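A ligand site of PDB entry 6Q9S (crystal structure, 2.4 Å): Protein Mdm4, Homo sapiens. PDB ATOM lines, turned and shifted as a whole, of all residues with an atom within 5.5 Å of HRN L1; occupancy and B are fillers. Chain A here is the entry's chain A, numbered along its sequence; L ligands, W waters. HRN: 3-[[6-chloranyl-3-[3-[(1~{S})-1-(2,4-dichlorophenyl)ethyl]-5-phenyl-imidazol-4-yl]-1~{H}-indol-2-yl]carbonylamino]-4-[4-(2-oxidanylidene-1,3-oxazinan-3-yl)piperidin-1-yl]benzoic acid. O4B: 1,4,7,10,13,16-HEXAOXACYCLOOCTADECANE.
The backbone carbonyl oxygen of Met 42 sits at hydrogen-bond distance from a nitrogen (N22) of HRN L1.
NE2 of His 43 is in hydrogen-bond range of O48 of HRN L1 (2.8 Å).
The backbone NH (N) of Val 81 lies within hydrogen-bond range of the backbone carbonyl oxygen (O) of His 61 (2.8 Å).
Lys 39 touches HRN L1 (CE to O48, 3.7 Å).
Leu 45 touches HRN L1 (CB to C31, 3.6 Å).
Gly 46 touches HRN L1 (CA to N22, 3.5 Å).
CD1 of Ile 49 touches C30 of HRN L1, at 3.6 Å.
Met 50 touches HRN L1 (CE to O76, 3.5 Å).
CE1 of Tyr 55 touches C70 of HRN L1, 3.6 Å away.
Gln 60 touches HRN L1.
Val 81 touches HRN L1 (O to C6, 3.5 Å).
Pro 84 touches HRN L1.
Leu 87 touches HRN L1.
CE2 of Tyr 88 touches CL2 of HRN L1, 3.96 Å away.
Hydrophobic or aromatic side chains within 4 Å of HRN L1: Met 42, His 43, Leu 45, Ile 49, Met 50, Tyr 55, Val 81, Leu 87 and Tyr 88.
Water W3 bridges O49 of HRN L1 and NZ of Lys 39.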
ATOM      1  N   LYS A  39     -32.585 -11.803  15.630  1.00  0.00           N
ATOM      2  CA  LYS A  39     -32.622 -13.198  15.155  1.00  0.00           C
ATOM      3  C   LYS A  39     -33.705 -13.443  14.089  1.00  0.00           C
ATOM      4  O   LYS A  39     -33.463 -14.117  13.090  1.00  0.00           O
ATOM      5  CB  LYS A  39     -32.785 -14.172  16.329  1.00  0.00           C
ATOM      6  CG  LYS A  39     -32.589 -15.633  15.967  1.00  0.00           C
ATOM      7  CD  LYS A  39     -32.801 -16.561  17.147  1.00  0.00           C
ATOM      8  CE  LYS A  39     -32.450 -17.970  16.770  1.00  0.00           C
ATOM      9  NZ  LYS A  39     -32.739 -18.951  17.862  1.00  0.00           N
ATOM     10  N   MET A  42     -32.658 -11.994  10.739  1.00  0.00           N
ATOM     11  CA  MET A  42     -31.739 -12.903  10.076  1.00  0.00           C
ATOM     12  C   MET A  42     -32.442 -14.149   9.549  1.00  0.00           C
ATOM     13  O   MET A  42     -32.140 -14.611   8.451  1.00  0.00           O
ATOM     14  CB  MET A  42     -30.589 -13.273  11.014  1.00  0.00           C
ATOM     15  CG  MET A  42     -29.921 -12.051  11.626  1.00  0.00           C
ATOM     16  SD  MET A  42     -28.459 -12.448  12.591  1.00  0.00           S
ATOM     17  CE  MET A  42     -27.182 -11.766  11.525  1.00  0.00           C
ATOM     18  N   HIS A  43     -33.399 -14.664  10.336  1.00  0.00           N
ATOM     19  CA  HIS A  43     -34.194 -15.816   9.926  1.00  0.00           C
ATOM     20  C   HIS A  43     -35.049 -15.527   8.695  1.00  0.00           C
ATOM     21  O   HIS A  43     -35.119 -16.353   7.790  1.00  0.00           O
ATOM     22  CB  HIS A  43     -35.041 -16.316  11.101  1.00  0.00           C
ATOM     23  CG  HIS A  43     -34.287 -17.182  12.067  1.00  0.00           C
ATOM     24  ND1 HIS A  43     -34.918 -17.984  12.991  1.00  0.00           N
ATOM     25  CD2 HIS A  43     -32.960 -17.408  12.216  1.00  0.00           C
ATOM     26  CE1 HIS A  43     -34.010 -18.653  13.687  1.00  0.00           C
ATOM     27  NE2 HIS A  43     -32.816 -18.311  13.237  1.00  0.00           N
ATOM     28  N   LEU A  45     -34.353 -13.108   6.415  1.00  0.00           N
ATOM     29  CA  LEU A  45     -33.427 -12.950   5.308  1.00  0.00           C
ATOM     30  C   LEU A  45     -33.005 -14.310   4.760  1.00  0.00           C
ATOM     31  O   LEU A  45     -32.945 -14.514   3.546  1.00  0.00           O
ATOM     32  CB  LEU A  45     -32.208 -12.110   5.706  1.00  0.00           C
ATOM     33  CG  LEU A  45     -32.493 -10.621   5.942  1.00  0.00           C
ATOM     34  CD1 LEU A  45     -31.377  -9.972   6.737  1.00  0.00           C
ATOM     35  CD2 LEU A  45     -32.725  -9.884   4.628  1.00  0.00           C
ATOM     36  N   GLY A  46     -32.742 -15.260   5.658  1.00  0.00           N
ATOM     37  CA  GLY A  46     -32.475 -16.640   5.258  1.00  0.00           C
ATOM     38  C   GLY A  46     -33.590 -17.240   4.399  1.00  0.00           C
ATOM     39  O   GLY A  46     -33.314 -17.897   3.397  1.00  0.00           O
ATOM     40  N   ILE A  49     -33.798 -15.492   0.935  1.00  0.00           N
ATOM     41  CA  ILE A  49     -32.786 -16.074   0.052  1.00  0.00           C
ATOM     42  C   ILE A  49     -33.229 -17.404  -0.550  1.00  0.00           C
ATOM     43  O   ILE A  49     -32.931 -17.695  -1.720  1.00  0.00           O
ATOM     44  CB  ILE A  49     -31.405 -16.205   0.767  1.00  0.00           C
ATOM     45  CG1 ILE A  49     -30.809 -14.821   1.002  1.00  0.00           C
ATOM     46  CG2 ILE A  49     -30.423 -17.114  -0.024  1.00  0.00           C
ATOM     47  CD1 ILE A  49     -29.698 -14.801   2.023  1.00  0.00           C
ATOM     48  N   MET A  50     -33.940 -18.209   0.241  1.00  0.00           N
ATOM     49  CA  MET A  50     -34.356 -19.538  -0.189  1.00  0.00           C
ATOM     50  C   MET A  50     -35.567 -19.534  -1.134  1.00  0.00           C
ATOM     51  O   MET A  50     -35.548 -20.241  -2.126  1.00  0.00           O
ATOM     52  CB  MET A  50     -34.570 -20.465   1.001  1.00  0.00           C
ATOM     53  CG  MET A  50     -33.267 -21.044   1.534  1.00  0.00           C
ATOM     54  SD  MET A  50     -33.510 -22.012   3.018  1.00  0.00           S
ATOM     55  CE  MET A  50     -33.685 -23.676   2.356  1.00  0.00           C
ATOM     56  N   TYR A  55     -29.244 -18.786  -3.494  1.00  0.00           N
ATOM     57  CA  TYR A  55     -28.058 -19.607  -3.217  1.00  0.00           C
ATOM     58  C   TYR A  55     -27.766 -20.661  -4.298  1.00  0.00           C
ATOM     59  O   TYR A  55     -28.605 -21.000  -5.101  1.00  0.00           O
ATOM     60  CB  TYR A  55     -28.146 -20.263  -1.833  1.00  0.00           C
ATOM     61  CG  TYR A  55     -29.202 -21.344  -1.724  1.00  0.00           C
ATOM     62  CD1 TYR A  55     -28.844 -22.686  -1.732  1.00  0.00           C
ATOM     63  CD2 TYR A  55     -30.550 -21.009  -1.625  1.00  0.00           C
ATOM     64  CE1 TYR A  55     -29.810 -23.677  -1.646  1.00  0.00           C
ATOM     65  CE2 TYR A  55     -31.515 -21.990  -1.540  1.00  0.00           C
ATOM     66  CZ  TYR A  55     -31.145 -23.314  -1.545  1.00  0.00           C
ATOM     67  OH  TYR A  55     -32.121 -24.283  -1.453  1.00  0.00           O
ATOM     68  N   GLN A  60     -23.981 -24.543  -1.107  1.00  0.00           N
ATOM     69  CA  GLN A  60     -24.909 -23.850  -0.219  1.00  0.00           C
ATOM     70  C   GLN A  60     -24.414 -22.537   0.417  1.00  0.00           C
ATOM     71  O   GLN A  60     -25.217 -21.621   0.634  1.00  0.00           O
ATOM     72  CB  GLN A  60     -25.353 -24.823   0.874  1.00  0.00           C
ATOM     73  CG  GLN A  60     -25.812 -24.147   2.191  1.00  0.00           C
ATOM     74  CD  GLN A  60     -25.299 -24.848   3.439  1.00  0.00           C
ATOM     75  OE1 GLN A  60     -24.990 -26.044   3.402  1.00  0.00           O
ATOM     76  NE2 GLN A  60     -25.219 -24.109   4.547  1.00  0.00           N
ATOM     77  N   HIS A  61     -23.137 -22.451   0.744  1.00  0.00           N
ATOM     78  CA  HIS A  61     -22.634 -21.287   1.483  1.00  0.00           C
ATOM     79  C   HIS A  61     -22.508 -20.030   0.625  1.00  0.00           C
ATOM     80  O   HIS A  61     -22.300 -18.936   1.149  1.00  0.00           O
ATOM     81  CB  HIS A  61     -21.320 -21.631   2.202  1.00  0.00           C
ATOM     82  CG  HIS A  61     -20.165 -21.858   1.286  1.00  0.00           C
ATOM     83  ND1 HIS A  61     -19.275 -20.864   0.933  1.00  0.00           N
ATOM     84  CD2 HIS A  61     -19.753 -22.978   0.641  1.00  0.00           C
ATOM     85  CE1 HIS A  61     -18.362 -21.352   0.114  1.00  0.00           C
ATOM     86  NE2 HIS A  61     -18.624 -22.634  -0.084  1.00  0.00           N
ATOM     87  N   VAL A  63     -24.169 -17.221  -1.730  1.00  0.00           N
ATOM     88  CA  VAL A  63     -25.399 -16.495  -2.034  1.00  0.00           C
ATOM     89  C   VAL A  63     -25.148 -15.522  -3.187  1.00  0.00           C
ATOM     90  O   VAL A  63     -24.168 -14.742  -3.176  1.00  0.00           O
ATOM     91  CB  VAL A  63     -25.904 -15.735  -0.785  1.00  0.00           C
ATOM     92  CG1 VAL A  63     -27.112 -14.882  -1.122  1.00  0.00           C
ATOM     93  CG2 VAL A  63     -26.222 -16.712   0.340  1.00  0.00           C
ATOM     94  N   LEU A  70     -32.050  -7.317  -2.393  1.00  0.00           N
ATOM     95  CA  LEU A  70     -31.091  -7.642  -1.340  1.00  0.00           C
ATOM     96  C   LEU A  70     -29.658  -7.278  -1.742  1.00  0.00           C
ATOM     97  O   LEU A  70     -28.882  -6.799  -0.910  1.00  0.00           O
ATOM     98  CB  LEU A  70     -31.194  -9.123  -0.951  1.00  0.00           C
ATOM     99  CG  LEU A  70     -30.219  -9.651   0.115  1.00  0.00           C
ATOM    100  CD1 LEU A  70     -30.493  -9.076   1.515  1.00  0.00           C
ATOM    101  CD2 LEU A  70     -30.232 -11.170   0.137  1.00  0.00           C
ATOM    102  N   LEU A  74     -27.165  -4.607   0.092  1.00  0.00           N
ATOM    103  CA  LEU A  74     -25.860  -5.055   0.598  1.00  0.00           C
ATOM    104  C   LEU A  74     -24.705  -4.433  -0.186  1.00  0.00           C
ATOM    105  O   LEU A  74     -23.541  -4.554   0.206  1.00  0.00           O
ATOM    106  CB  LEU A  74     -25.754  -6.580   0.515  1.00  0.00           C
ATOM    107  CG  LEU A  74     -26.627  -7.414   1.442  1.00  0.00           C
ATOM    108  CD1 LEU A  74     -26.748  -8.821   0.884  1.00  0.00           C
ATOM    109  CD2 LEU A  74     -26.044  -7.435   2.839  1.00  0.00           C
ATOM    110  N   PHE A  79     -21.854 -13.211  -2.000  1.00  0.00           N
ATOM    111  CA  PHE A  79     -21.069 -13.331  -0.785  1.00  0.00           C
ATOM    112  C   PHE A  79     -21.164 -14.739  -0.232  1.00  0.00           C
ATOM    113  O   PHE A  79     -22.146 -15.442  -0.485  1.00  0.00           O
ATOM    114  CB  PHE A  79     -21.485 -12.292   0.286  1.00  0.00           C
ATOM    115  CG  PHE A  79     -22.879 -12.507   0.845  1.00  0.00           C
ATOM    116  CD1 PHE A  79     -23.060 -13.207   2.043  1.00  0.00           C
ATOM    117  CD2 PHE A  79     -23.996 -11.984   0.207  1.00  0.00           C
ATOM    118  CE1 PHE A  79     -24.340 -13.395   2.577  1.00  0.00           C
ATOM    119  CE2 PHE A  79     -25.273 -12.163   0.732  1.00  0.00           C
ATOM    120  CZ  PHE A  79     -25.442 -12.874   1.922  1.00  0.00           C
ATOM    121  N   VAL A  81     -21.638 -17.052   3.089  1.00  0.00           N
ATOM    122  CA  VAL A  81     -22.285 -16.928   4.407  1.00  0.00           C
ATOM    123  C   VAL A  81     -21.279 -17.105   5.546  1.00  0.00           C
ATOM    124  O   VAL A  81     -21.600 -16.922   6.716  1.00  0.00           O
ATOM    125  CB  VAL A  81     -23.496 -17.897   4.606  1.00  0.00           C
ATOM    126  CG1 VAL A  81     -24.533 -17.735   3.500  1.00  0.00           C
ATOM    127  CG2 VAL A  81     -23.036 -19.359   4.753  1.00  0.00           C
ATOM    128  N   PRO A  84     -19.774 -12.908   7.778  1.00  0.00           N
ATOM    129  CA  PRO A  84     -20.804 -11.999   8.309  1.00  0.00           C
ATOM    130  C   PRO A  84     -20.714 -10.549   7.836  1.00  0.00           C
ATOM    131  O   PRO A  84     -21.745  -9.906   7.647  1.00  0.00           O
ATOM    132  CB  PRO A  84     -20.568 -12.046   9.837  1.00  0.00           C
ATOM    133  CG  PRO A  84     -19.415 -12.995  10.061  1.00  0.00           C
ATOM    134  CD  PRO A  84     -19.308 -13.829   8.829  1.00  0.00           C
ATOM    135  N   LEU A  87     -23.344  -8.443   5.788  1.00  0.00           N
ATOM    136  CA  LEU A  87     -24.650  -8.536   6.425  1.00  0.00           C
ATOM    137  C   LEU A  87     -24.756  -7.651   7.675  1.00  0.00           C
ATOM    138  O   LEU A  87     -25.633  -6.810   7.742  1.00  0.00           O
ATOM    139  CB  LEU A  87     -25.009  -9.998   6.728  1.00  0.00           C
ATOM    140  CG  LEU A  87     -26.514 -10.321   6.779  1.00  0.00           C
ATOM    141  CD1 LEU A  87     -27.009 -10.454   8.200  1.00  0.00           C
ATOM    142  CD2 LEU A  87     -27.354  -9.289   6.020  1.00  0.00           C
ATOM    143  N   TYR A  88     -23.841  -7.862   8.628  1.00  0.00           N
ATOM    144  CA  TYR A  88     -23.786  -7.058   9.861  1.00  0.00           C
ATOM    145  C   TYR A  88     -23.739  -5.548   9.580  1.00  0.00           C
ATOM    146  O   TYR A  88     -24.483  -4.782  10.190  1.00  0.00           O
ATOM    147  CB  TYR A  88     -22.596  -7.485  10.739  1.00  0.00           C
ATOM    148  CG  TYR A  88     -22.819  -8.730  11.582  1.00  0.00           C
ATOM    149  CD1 TYR A  88     -22.445  -8.767  12.937  1.00  0.00           C
ATOM    150  CD2 TYR A  88     -23.414  -9.889  11.036  1.00  0.00           C
ATOM    151  CE1 TYR A  88     -22.645  -9.916  13.729  1.00  0.00           C
ATOM    152  CE2 TYR A  88     -23.621 -11.037  11.816  1.00  0.00           C
ATOM    153  CZ  TYR A  88     -23.229 -11.047  13.154  1.00  0.00           C
ATOM    154  OH  TYR A  88     -23.437 -12.185  13.902  1.00  0.00           O
HETATM  155  C2  HRN L   1     -26.773 -16.291   9.864  1.00  0.00           C
HETATM  156  C3  HRN L   1     -26.231 -17.368   9.136  1.00  0.00           C
HETATM  157  C42 HRN L   1     -30.558 -22.463  12.021  1.00  0.00           C
HETATM  158  C44 HRN L   1     -30.411 -21.114  12.372  1.00  0.00           C
HETATM  159  C45 HRN L   1     -30.191 -20.153  11.378  1.00  0.00           C
HETATM  160  C47 HRN L   1     -30.465 -20.685  13.823  1.00  0.00           C
HETATM  161  C52 HRN L   1     -31.485 -22.421   7.646  1.00  0.00           C
HETATM  162  C55 HRN L   1     -31.349 -22.660   6.123  1.00  0.00           C
HETATM  163  C58 HRN L   1     -30.266 -23.731   5.882  1.00  0.00           C
HETATM  164  C60 HRN L   1     -28.910 -23.227   6.445  1.00  0.00           C
HETATM  165  C12 HRN L   1     -26.832 -18.773   9.313  1.00  0.00           C
HETATM  166  C15 HRN L   1     -26.349 -20.447   7.578  1.00  0.00           C
HETATM  167  C18 HRN L   1     -27.582 -19.699   5.920  1.00  0.00           C
HETATM  168  C19 HRN L   1     -27.738 -18.913   6.997  1.00  0.00           C
HETATM  169  C20 HRN L   1     -28.586 -17.702   7.115  1.00  0.00           C
HETATM  170  C21 HRN L   1     -29.665 -17.416   7.883  1.00  0.00           C
HETATM  171  C24 HRN L   1     -29.255 -15.585   6.737  1.00  0.00           C
HETATM  172  C25 HRN L   1     -28.280 -16.465   6.314  1.00  0.00           C
HETATM  173  C26 HRN L   1     -27.330 -16.135   5.349  1.00  0.00           C
HETATM  174  C28 HRN L   1     -27.397 -14.838   4.813  1.00  0.00           C
HETATM  175  C30 HRN L   1     -28.383 -13.936   5.252  1.00  0.00           C
HETATM  176 CL1  HRN L   1     -28.082 -16.524  11.012  1.00  0.00          CL
HETATM  177  C4  HRN L   1     -25.190 -17.138   8.219  1.00  0.00           C
HETATM  178  C6  HRN L   1     -24.672 -15.853   8.068  1.00  0.00           C
HETATM  179  C8  HRN L   1     -25.211 -14.807   8.809  1.00  0.00           C
HETATM  180  C9  HRN L   1     -26.254 -15.016   9.703  1.00  0.00           C
HETATM  181 CL2  HRN L   1     -24.575 -13.194   8.629  1.00  0.00          CL
HETATM  182  N14 HRN L   1     -26.973 -19.378   7.977  1.00  0.00           N
HETATM  183  N17 HRN L   1     -26.668 -20.695   6.406  1.00  0.00           N
HETATM  184  N22 HRN L   1     -30.019 -16.179   7.669  1.00  0.00           N
HETATM  185  C31 HRN L   1     -29.337 -14.296   6.218  1.00  0.00           C
HETATM  186 CL3  HRN L   1     -28.437 -12.312   4.569  1.00  0.00          CL
HETATM  187  C34 HRN L   1     -30.288 -18.278   8.915  1.00  0.00           C
HETATM  188  O35 HRN L   1     -31.109 -17.771   9.664  1.00  0.00           O
HETATM  189  N36 HRN L   1     -29.845 -19.547   9.049  1.00  0.00           N
HETATM  190  C38 HRN L   1     -30.144 -20.519  10.024  1.00  0.00           C
HETATM  191  C39 HRN L   1     -30.248 -21.853   9.673  1.00  0.00           C
HETATM  192  C40 HRN L   1     -30.489 -22.831  10.663  1.00  0.00           C
HETATM  193  O48 HRN L   1     -30.474 -19.500  14.102  1.00  0.00           O
HETATM  194  O49 HRN L   1     -30.444 -21.615  14.784  1.00  0.00           O
HETATM  195  N51 HRN L   1     -30.177 -22.201   8.315  1.00  0.00           N
HETATM  196  C63 HRN L   1     -29.024 -23.071   7.967  1.00  0.00           C
HETATM  197  N66 HRN L   1     -30.228 -24.067   4.452  1.00  0.00           N
HETATM  198  C67 HRN L   1     -29.571 -23.188   3.459  1.00  0.00           C
HETATM  199  C70 HRN L   1     -29.859 -23.557   1.990  1.00  0.00           C
HETATM  200  C73 HRN L   1     -29.827 -25.093   1.911  1.00  0.00           C
HETATM  201  O76 HRN L   1     -30.832 -25.661   2.781  1.00  0.00           O
HETATM  202  C77 HRN L   1     -30.811 -25.244   4.056  1.00  0.00           C
HETATM  203  O78 HRN L   1     -31.345 -26.000   4.868  1.00  0.00           O
HETATM  204  C79 HRN L   1     -28.199 -19.754   4.539  1.00  0.00           C
HETATM  205  C80 HRN L   1     -27.425 -20.311   3.502  1.00  0.00           C
HETATM  206  C82 HRN L   1     -27.944 -20.417   2.200  1.00  0.00           C
HETATM  207  C84 HRN L   1     -29.249 -19.984   1.933  1.00  0.00           C
HETATM  208  C86 HRN L   1     -30.035 -19.446   2.967  1.00  0.00           C
HETATM  209  C88 HRN L   1     -29.514 -19.341   4.260  1.00  0.00           C
HETATM  210  C90 HRN L   1     -26.059 -19.620  10.335  1.00  0.00           C
HETATM  211  CAA O4B L   2     -22.456 -20.371   8.471  1.00  0.00           C
HETATM  212  OAM O4B L   2     -22.897 -21.408   9.362  1.00  0.00           O
HETATM  213  CAC O4B L   2     -23.532 -22.485   8.647  1.00  0.00           C
HETATM  214  CAD O4B L   2     -24.003 -23.587   9.627  1.00  0.00           C
HETATM  215  OAO O4B L   2     -25.346 -23.296  10.090  1.00  0.00           O
HETATM  216  CAG O4B L   2     -25.649 -23.980  11.329  1.00  0.00           C
HETATM  217  CAH O4B L   2     -26.825 -23.281  12.051  1.00  0.00           C
HETATM  218  OAQ O4B L   2     -26.339 -22.126  12.775  1.00  0.00           O
HETATM  219  CAK O4B L   2     -27.202 -21.749  13.871  1.00  0.00           C
HETATM  220  CAL O4B L   2     -26.638 -20.570  14.707  1.00  0.00           C
HETATM  221  OAR O4B L   2     -26.087 -19.576  13.815  1.00  0.00           O
HETATM  222  CAJ O4B L   2     -25.343 -18.533  14.497  1.00  0.00           C
HETATM  223  CAI O4B L   2     -24.799 -17.500  13.487  1.00  0.00           C
HETATM  224  OAP O4B L   2     -23.756 -18.105  12.675  1.00  0.00           O
HETATM  225  CAF O4B L   2     -22.858 -17.137  12.078  1.00  0.00           C
HETATM  226  CAE O4B L   2     -22.507 -17.531  10.617  1.00  0.00           C
HETATM  227  OAN O4B L   2     -22.305 -18.957  10.492  1.00  0.00           O
HETATM  228  CAB O4B L   2     -21.661 -19.301   9.246  1.00  0.00           C
HETATM  229  CAA O4B L   3     -36.602 -24.011  12.861  1.00  0.00           C
HETATM  230  OAM O4B L   3     -35.925 -23.113  11.964  1.00  0.00           O
HETATM  231  CAC O4B L   3     -34.892 -22.327  12.576  1.00  0.00           C
HETATM  232  CAD O4B L   3     -33.930 -21.830  11.482  1.00  0.00           C
HETATM  233  OAO O4B L   3     -34.534 -20.755  10.750  1.00  0.00           O
HETATM  234  CAG O4B L   3     -33.719 -20.280   9.651  1.00  0.00           C
HETATM  235  CAH O4B L   3     -34.613 -19.693   8.539  1.00  0.00           C
HETATM  236  OAQ O4B L   3     -34.752 -20.664   7.480  1.00  0.00           O
HETATM  237  CAK O4B L   3     -35.780 -20.309   6.543  1.00  0.00           C
HETATM  238  CAL O4B L   3     -36.302 -21.561   5.793  1.00  0.00           C
HETATM  239  OAR O4B L   3     -36.833 -22.496   6.760  1.00  0.00           O
HETATM  240  CAJ O4B L   3     -38.264 -22.678   6.709  1.00  0.00           C
HETATM  241  CAI O4B L   3     -38.587 -24.191   6.724  1.00  0.00           C
HETATM  242  OAP O4B L   3     -38.292 -24.794   8.016  1.00  0.00           O
HETATM  243  CAF O4B L   3     -39.417 -24.792   8.920  1.00  0.00           C
HETATM  244  CAE O4B L   3     -39.089 -23.970  10.190  1.00  0.00           C
HETATM  245  OAN O4B L   3     -38.037 -24.624  10.941  1.00  0.00           O
HETATM  246  CAB O4B L   3     -38.046 -24.262  12.346  1.00  0.00           C
HETATM  247  O   HOH W   1     -29.036 -24.333  14.728  1.00  0.00           O
HETATM  248  O   HOH W   2     -31.435 -28.710   1.348  1.00  0.00           O
HETATM  249  O   HOH W   3     -32.057 -21.253  16.652  1.00  0.00           O
